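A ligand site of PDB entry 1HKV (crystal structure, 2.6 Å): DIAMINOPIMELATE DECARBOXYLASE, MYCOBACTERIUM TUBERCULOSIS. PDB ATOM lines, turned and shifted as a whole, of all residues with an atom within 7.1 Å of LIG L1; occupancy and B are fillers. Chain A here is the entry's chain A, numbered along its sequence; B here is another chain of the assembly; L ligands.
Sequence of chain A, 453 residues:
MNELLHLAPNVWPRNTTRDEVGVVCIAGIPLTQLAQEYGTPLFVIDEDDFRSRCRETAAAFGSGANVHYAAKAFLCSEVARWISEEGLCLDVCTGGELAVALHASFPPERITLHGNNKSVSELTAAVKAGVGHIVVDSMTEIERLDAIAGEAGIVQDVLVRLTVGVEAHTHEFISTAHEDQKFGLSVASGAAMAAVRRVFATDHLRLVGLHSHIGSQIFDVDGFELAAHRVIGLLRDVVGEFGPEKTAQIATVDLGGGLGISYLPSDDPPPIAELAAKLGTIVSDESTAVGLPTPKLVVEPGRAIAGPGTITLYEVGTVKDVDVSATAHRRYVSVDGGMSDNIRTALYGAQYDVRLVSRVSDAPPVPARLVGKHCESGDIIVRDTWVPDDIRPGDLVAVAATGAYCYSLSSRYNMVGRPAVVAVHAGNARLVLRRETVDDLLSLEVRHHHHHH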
ATOM      1  N   LYS A  72      -3.228  26.398  24.464  1.00  0.00           N
ATOM      2  CA  LYS A  72      -3.347  25.148  25.210  1.00  0.00           C
ATOM      3  C   LYS A  72      -4.016  24.074  24.325  1.00  0.00           C
ATOM      4  O   LYS A  72      -3.775  22.894  24.519  1.00  0.00           O
ATOM      5  CB  LYS A  72      -4.141  25.378  26.465  1.00  0.00           C
ATOM      6  CG  LYS A  72      -5.494  26.131  26.199  1.00  0.00           C
ATOM      7  CD  LYS A  72      -6.121  26.659  27.482  1.00  0.00           C
ATOM      8  CE  LYS A  72      -7.097  25.691  28.083  1.00  0.00           C
ATOM      9  NZ  LYS A  72      -8.357  26.437  28.261  1.00  0.00           N
ATOM     10  N   HIS A 169     -22.339  25.324  28.503  1.00  0.00           N
ATOM     11  CA  HIS A 169     -21.976  24.090  27.752  1.00  0.00           C
ATOM     12  C   HIS A 169     -23.058  23.710  26.828  1.00  0.00           C
ATOM     13  O   HIS A 169     -24.185  23.629  27.210  1.00  0.00           O
ATOM     14  CB  HIS A 169     -21.676  22.859  28.663  1.00  0.00           C
ATOM     15  CG  HIS A 169     -20.521  23.043  29.612  1.00  0.00           C
ATOM     16  ND1 HIS A 169     -19.210  23.215  29.175  1.00  0.00           N
ATOM     17  CD2 HIS A 169     -20.468  23.046  30.967  1.00  0.00           C
ATOM     18  CE1 HIS A 169     -18.412  23.344  30.233  1.00  0.00           C
ATOM     19  NE2 HIS A 169     -19.145  23.237  31.327  1.00  0.00           N
ATOM     20  N   THR A 170     -22.680  23.415  25.616  1.00  0.00           N
ATOM     21  CA  THR A 170     -23.600  23.176  24.517  1.00  0.00           C
ATOM     22  C   THR A 170     -24.776  24.105  24.598  1.00  0.00           C
ATOM     23  O   THR A 170     -24.586  25.330  24.420  1.00  0.00           O
ATOM     24  CB  THR A 170     -23.965  21.629  24.419  1.00  0.00           C
ATOM     25  OG1 THR A 170     -24.431  21.136  25.656  1.00  0.00           O
ATOM     26  CG2 THR A 170     -22.692  20.789  24.241  1.00  0.00           C
ATOM     27  N   PHE A 183     -10.123  30.338  39.245  1.00  0.00           N
ATOM     28  CA  PHE A 183      -9.816  31.482  38.420  1.00  0.00           C
ATOM     29  C   PHE A 183     -10.604  32.698  38.857  1.00  0.00           C
ATOM     30  O   PHE A 183     -11.766  32.596  39.360  1.00  0.00           O
ATOM     31  CB  PHE A 183     -10.134  31.221  36.900  1.00  0.00           C
ATOM     32  CG  PHE A 183      -9.134  30.353  36.228  1.00  0.00           C
ATOM     33  CD1 PHE A 183      -7.888  30.837  35.883  1.00  0.00           C
ATOM     34  CD2 PHE A 183      -9.426  29.007  35.931  1.00  0.00           C
ATOM     35  CE1 PHE A 183      -6.929  30.009  35.256  1.00  0.00           C
ATOM     36  CE2 PHE A 183      -8.506  28.207  35.353  1.00  0.00           C
ATOM     37  CZ  PHE A 183      -7.234  28.722  34.997  1.00  0.00           C
ATOM     38  N   HIS A 213     -14.015  34.063  31.186  1.00  0.00           N
ATOM     39  CA  HIS A 213     -14.092  32.803  30.444  1.00  0.00           C
ATOM     40  C   HIS A 213     -15.091  31.900  31.090  1.00  0.00           C
ATOM     41  O   HIS A 213     -14.927  31.556  32.236  1.00  0.00           O
ATOM     42  CB  HIS A 213     -12.717  32.102  30.412  1.00  0.00           C
ATOM     43  CG  HIS A 213     -12.718  30.802  29.634  1.00  0.00           C
ATOM     44  ND1 HIS A 213     -13.029  30.758  28.284  1.00  0.00           N
ATOM     45  CD2 HIS A 213     -12.453  29.524  30.021  1.00  0.00           C
ATOM     46  CE1 HIS A 213     -12.932  29.507  27.868  1.00  0.00           C
ATOM     47  NE2 HIS A 213     -12.588  28.746  28.899  1.00  0.00           N
ATOM     48  N   GLY A 215     -16.859  28.744  29.720  1.00  0.00           N
ATOM     49  CA  GLY A 215     -17.122  27.342  29.410  1.00  0.00           C
ATOM     50  C   GLY A 215     -16.432  26.735  28.190  1.00  0.00           C
ATOM     51  O   GLY A 215     -15.424  27.187  27.717  1.00  0.00           O
ATOM     52  N   SER A 216     -16.964  25.636  27.733  1.00  0.00           N
ATOM     53  CA  SER A 216     -16.500  25.076  26.521  1.00  0.00           C
ATOM     54  C   SER A 216     -17.624  24.401  25.779  1.00  0.00           C
ATOM     55  O   SER A 216     -18.605  24.103  26.355  1.00  0.00           O
ATOM     56  CB  SER A 216     -15.435  24.121  26.816  1.00  0.00           C
ATOM     57  OG  SER A 216     -16.025  23.033  27.422  1.00  0.00           O
ATOM     58  N   GLN A 217     -17.445  24.192  24.480  1.00  0.00           N
ATOM     59  CA  GLN A 217     -18.409  23.514  23.612  1.00  0.00           C
ATOM     60  C   GLN A 217     -19.781  24.214  23.634  1.00  0.00           C
ATOM     61  O   GLN A 217     -20.807  23.605  23.513  1.00  0.00           O
ATOM     62  CB  GLN A 217     -18.522  22.010  23.988  1.00  0.00           C
ATOM     63  CG  GLN A 217     -17.576  21.079  23.148  1.00  0.00           C
ATOM     64  CD  GLN A 217     -17.790  21.255  21.601  1.00  0.00           C
ATOM     65  OE1 GLN A 217     -17.220  22.162  20.993  1.00  0.00           O
ATOM     66  NE2 GLN A 217     -18.589  20.397  21.009  1.00  0.00           N
ATOM     67  N   TYR A 263     -18.133  17.618  17.085  1.00  0.00           N
ATOM     68  CA  TYR A 263     -17.563  16.295  17.190  1.00  0.00           C
ATOM     69  C   TYR A 263     -18.421  15.197  16.493  1.00  0.00           C
ATOM     70  O   TYR A 263     -17.897  14.185  16.012  1.00  0.00           O
ATOM     71  CB  TYR A 263     -17.405  15.961  18.669  1.00  0.00           C
ATOM     72  CG  TYR A 263     -16.276  16.679  19.309  1.00  0.00           C
ATOM     73  CD1 TYR A 263     -16.492  17.872  20.000  1.00  0.00           C
ATOM     74  CD2 TYR A 263     -14.929  16.213  19.172  1.00  0.00           C
ATOM     75  CE1 TYR A 263     -15.443  18.570  20.550  1.00  0.00           C
ATOM     76  CE2 TYR A 263     -13.876  16.934  19.750  1.00  0.00           C
ATOM     77  CZ  TYR A 263     -14.148  18.091  20.423  1.00  0.00           C
ATOM     78  OH  TYR A 263     -13.180  18.821  21.010  1.00  0.00           O
ATOM     79  N   ARG A 303     -10.206  25.614  20.545  1.00  0.00           N
ATOM     80  CA  ARG A 303     -10.757  24.499  19.876  1.00  0.00           C
ATOM     81  C   ARG A 303     -11.359  24.825  18.549  1.00  0.00           C
ATOM     82  O   ARG A 303     -11.265  24.040  17.644  1.00  0.00           O
ATOM     83  CB  ARG A 303     -11.853  23.935  20.779  1.00  0.00           C
ATOM     84  CG  ARG A 303     -12.607  22.744  20.272  1.00  0.00           C
ATOM     85  CD  ARG A 303     -13.802  22.357  21.220  1.00  0.00           C
ATOM     86  NE  ARG A 303     -13.412  21.505  22.364  1.00  0.00           N
ATOM     87  CZ  ARG A 303     -13.191  21.936  23.575  1.00  0.00           C
ATOM     88  NH1 ARG A 303     -12.863  21.098  24.512  1.00  0.00           N
ATOM     89  NH2 ARG A 303     -13.290  23.186  23.865  1.00  0.00           N
ATOM     90  N   ARG A 344      -9.633  12.194  26.057  1.00  0.00           N
ATOM     91  CA  ARG A 344     -10.743  13.104  26.231  1.00  0.00           C
ATOM     92  C   ARG A 344     -11.968  12.339  26.584  1.00  0.00           C
ATOM     93  O   ARG A 344     -12.775  12.786  27.364  1.00  0.00           O
ATOM     94  CB  ARG A 344     -10.989  13.940  24.980  1.00  0.00           C
ATOM     95  CG  ARG A 344     -10.052  15.175  24.884  1.00  0.00           C
ATOM     96  CD  ARG A 344     -10.540  16.220  23.972  1.00  0.00           C
ATOM     97  NE  ARG A 344     -11.692  16.851  24.524  1.00  0.00           N
ATOM     98  CZ  ARG A 344     -12.880  16.794  24.015  1.00  0.00           C
ATOM     99  NH1 ARG A 344     -13.124  16.115  22.888  1.00  0.00           N
ATOM    100  NH2 ARG A 344     -13.854  17.438  24.621  1.00  0.00           N
ATOM    101  N   TYR A 348     -13.265  13.527  30.056  1.00  0.00           N
ATOM    102  CA  TYR A 348     -14.396  14.435  30.015  1.00  0.00           C
ATOM    103  C   TYR A 348     -15.727  13.750  29.528  1.00  0.00           C
ATOM    104  O   TYR A 348     -16.722  14.417  29.369  1.00  0.00           O
ATOM    105  CB  TYR A 348     -14.091  15.553  29.048  1.00  0.00           C
ATOM    106  CG  TYR A 348     -12.813  16.307  29.330  1.00  0.00           C
ATOM    107  CD1 TYR A 348     -11.803  16.396  28.340  1.00  0.00           C
ATOM    108  CD2 TYR A 348     -12.593  16.908  30.581  1.00  0.00           C
ATOM    109  CE1 TYR A 348     -10.679  17.060  28.569  1.00  0.00           C
ATOM    110  CE2 TYR A 348     -11.479  17.580  30.817  1.00  0.00           C
ATOM    111  CZ  TYR A 348     -10.510  17.672  29.806  1.00  0.00           C
ATOM    112  OH  TYR A 348      -9.368  18.336  30.019  1.00  0.00           O
ATOM    113  N   ALA A 350     -16.122  12.749  26.505  1.00  0.00           N
ATOM    114  CA  ALA A 350     -16.336  13.270  25.176  1.00  0.00           C
ATOM    115  C   ALA A 350     -16.865  12.183  24.234  1.00  0.00           C
ATOM    116  O   ALA A 350     -16.728  11.051  24.487  1.00  0.00           O
ATOM    117  CB  ALA A 350     -15.070  13.894  24.630  1.00  0.00           C
ATOM    118  N   TYR A 405      -6.761  19.629  22.033  1.00  0.00           N
ATOM    119  CA  TYR A 405      -6.710  19.050  23.354  1.00  0.00           C
ATOM    120  C   TYR A 405      -6.224  17.638  23.392  1.00  0.00           C
ATOM    121  O   TYR A 405      -5.745  17.197  24.438  1.00  0.00           O
ATOM    122  CB  TYR A 405      -8.040  19.287  24.169  1.00  0.00           C
ATOM    123  CG  TYR A 405      -8.235  20.785  24.450  1.00  0.00           C
ATOM    124  CD1 TYR A 405      -7.414  21.476  25.353  1.00  0.00           C
ATOM    125  CD2 TYR A 405      -9.154  21.510  23.732  1.00  0.00           C
ATOM    126  CE1 TYR A 405      -7.536  22.910  25.528  1.00  0.00           C
ATOM    127  CE2 TYR A 405      -9.274  22.906  23.905  1.00  0.00           C
ATOM    128  CZ  TYR A 405      -8.468  23.571  24.798  1.00  0.00           C
ATOM    129  OH  TYR A 405      -8.657  24.856  24.954  1.00  0.00           O
ATOM    130  N   CYS B 375      -4.316  26.165  32.649  1.00  0.00           N
ATOM    131  CA  CYS B 375      -5.439  27.025  32.305  1.00  0.00           C
ATOM    132  C   CYS B 375      -6.735  26.249  32.096  1.00  0.00           C
ATOM    133  O   CYS B 375      -7.390  26.387  31.075  1.00  0.00           O
ATOM    134  CB  CYS B 375      -5.155  27.850  31.074  1.00  0.00           C
ATOM    135  SG  CYS B 375      -4.152  29.207  31.453  1.00  0.00           S
ATOM    136  N   GLU B 376      -7.137  25.502  33.114  1.00  0.00           N
ATOM    137  CA  GLU B 376      -8.312  24.730  33.060  1.00  0.00           C
ATOM    138  C   GLU B 376      -8.922  24.594  34.475  1.00  0.00           C
ATOM    139  O   GLU B 376      -8.218  24.214  35.408  1.00  0.00           O
ATOM    140  CB  GLU B 376      -7.937  23.358  32.496  1.00  0.00           C
ATOM    141  CG  GLU B 376      -9.120  22.453  32.162  1.00  0.00           C
ATOM    142  CD  GLU B 376      -8.698  21.191  31.473  1.00  0.00           C
ATOM    143  OE1 GLU B 376      -8.185  21.303  30.333  1.00  0.00           O
ATOM    144  OE2 GLU B 376      -8.855  20.098  32.064  1.00  0.00           O
ATOM    145  N   SER B 377     -10.216  24.866  34.631  1.00  0.00           N
ATOM    146  CA  SER B 377     -10.800  24.881  35.981  1.00  0.00           C
ATOM    147  C   SER B 377     -10.716  23.599  36.669  1.00  0.00           C
ATOM    148  O   SER B 377     -10.629  23.576  37.923  1.00  0.00           O
ATOM    149  CB  SER B 377     -12.202  25.259  35.943  1.00  0.00           C
ATOM    150  OG  SER B 377     -12.325  26.521  35.354  1.00  0.00           O
ATOM    151  N   GLY B 378     -10.745  22.476  35.882  1.00  0.00           N
ATOM    152  CA  GLY B 378     -10.724  21.139  36.470  1.00  0.00           C
ATOM    153  C   GLY B 378      -9.347  20.676  36.886  1.00  0.00           C
ATOM    154  O   GLY B 378      -9.129  19.514  37.207  1.00  0.00           O
ATOM    155  N   TYR B 413       0.846  19.022  29.590  1.00  0.00           N
ATOM    156  CA  TYR B 413      -0.275  19.970  29.397  1.00  0.00           C
ATOM    157  C   TYR B 413       0.219  21.347  29.718  1.00  0.00           C
ATOM    158  O   TYR B 413       0.915  21.569  30.742  1.00  0.00           O
ATOM    159  CB  TYR B 413      -1.489  19.582  30.256  1.00  0.00           C
ATOM    160  CG  TYR B 413      -2.793  20.275  29.857  1.00  0.00           C
ATOM    161  CD1 TYR B 413      -3.730  20.584  30.799  1.00  0.00           C
ATOM    162  CD2 TYR B 413      -3.079  20.579  28.530  1.00  0.00           C
ATOM    163  CE1 TYR B 413      -4.942  21.252  30.448  1.00  0.00           C
ATOM    164  CE2 TYR B 413      -4.290  21.244  28.169  1.00  0.00           C
ATOM    165  CZ  TYR B 413      -5.212  21.569  29.164  1.00  0.00           C
ATOM    166  OH  TYR B 413      -6.441  22.200  28.858  1.00  0.00           O
HETATM  167  N1  LIG L   1     -15.298  20.035  29.810  1.00  0.00           N
HETATM  168  C1  LIG L   1     -14.674  20.589  28.602  1.00  0.00           C
HETATM  169  C2  LIG L   1     -15.064  19.802  27.333  1.00  0.00           C
HETATM  170  O1  LIG L   1     -16.236  19.833  26.905  1.00  0.00           O
HETATM  171  C3  LIG L   1     -13.102  20.679  28.761  1.00  0.00           C
HETATM  172  C4  LIG L   1     -12.559  22.141  28.973  1.00  0.00           C
HETATM  173  C5  LIG L   1     -11.129  22.350  28.423  1.00  0.00           C
HETATM  174  C6  LIG L   1     -10.403  23.660  29.046  1.00  0.00           C
HETATM  175  N2  LIG L   1     -11.269  24.623  29.932  1.00  0.00           N
HETATM  176  O2  LIG L   1     -14.218  19.135  26.689  1.00  0.00           O
HETATM  177  N1  LG2 L   2      -9.465  31.495  27.269  1.00  0.00           N
HETATM  178  C1  LG2 L   2      -9.073  30.911  28.487  1.00  0.00           C
HETATM  179  C2  LG2 L   2      -8.772  31.783  29.675  1.00  0.00           C
HETATM  180  C3  LG2 L   2      -8.953  29.545  28.603  1.00  0.00           C
HETATM  181  O1  LG2 L   2      -8.551  29.027  29.811  1.00  0.00           O
HETATM  182  C4  LG2 L   2      -9.186  28.726  27.495  1.00  0.00           C
HETATM  183  C5  LG2 L   2      -9.046  27.334  27.610  1.00  0.00           C
HETATM  184  C6  LG2 L   2      -9.573  29.294  26.270  1.00  0.00           C
HETATM  185  C7  LG2 L   2      -9.708  30.694  26.155  1.00  0.00           C
HETATM  186  C8  LG2 L   2      -9.889  28.419  25.048  1.00  0.00           C
HETATM  187  O2  LG2 L   2     -10.916  27.454  25.226  1.00  0.00           O
HETATM  188  P1  LG2 L   2     -11.645  26.693  23.993  1.00  0.00           P
HETATM  189  O3  LG2 L   2     -12.830  26.013  24.559  1.00  0.00           O
HETATM  190  O4  LG2 L   2     -10.715  25.596  23.495  1.00  0.00           O
HETATM  191  O5  LG2 L   2     -12.184  27.635  22.899  1.00  0.00           O
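Residues that only touch LIG L1: Lys 72 (3.5 Å) and Glu 376 of chain B (3.5 Å). Of the 19 residues printed, 5 come within 4 Å of LIG L1. The nearest printed residue that does not touch LIG L1 is Tyr 348 (4.01 Å).
NH2 of Arg 344 is in salt-bridge range of O2 of LIG L1. The side-chain hydroxyl (OG) of Ser 216 lies close to an oxygen (O1) of LIG L1. O2 of LIG L1 lies within salt-bridge range of NH1 of Arg 303, 3.2 Å away. An oxygen (O4) of LG2 L2 sits at hydrogen-bond distance from the backbone NH (N) of Arg 303 (3.0 Å). The guanidinium group of Arg 303 lies within salt-bridge range of an oxygen (O3) of LG2 L2, at 2.9 Å. NZ of Lys 72 is covalently linked to C5 of LG2 L2, 1.3 Å away. An oxygen (O1) of LG2 L2 lies within hydrogen-bond range of the backbone carbonyl oxygen (O) of Cys 375 of chain B. OH of Tyr 405 lies within hydrogen-bond range of O4 of LG2 L2, at 2.6 Å.
O of Arg 344 lies within hydrogen-bond range of N of Ala 350 (3.5 Å). The side-chain hydroxyl of Tyr 263 is in hydrogen-bond range of the guanidinium group of Arg 344 (3.3 Å). The backbone carbonyl oxygen (O) of Ser 216 sits at hydrogen-bond distance from a ring nitrogen (ND1) of His 169 (3.0 Å). OH of Tyr 263 sits at hydrogen-bond distance from NE of Arg 303, at 3.0 Å. The side-chain hydroxyl (OH) of Tyr 348 is in hydrogen-bond range of the side-chain carboxylate (OE2) of Glu 376 of chain B (2.7 Å). The side-chain carboxylate (OE1) of Glu 376 of chain B sits at hydrogen-bond distance from the side-chain hydroxyl (OH) of Tyr 413 of chain B (2.5 Å). The backbone carbonyl oxygen (O) of Cys 375 of chain B lies within hydrogen-bond range of the side-chain amino group (NZ) of Lys 72 (3.0 Å).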
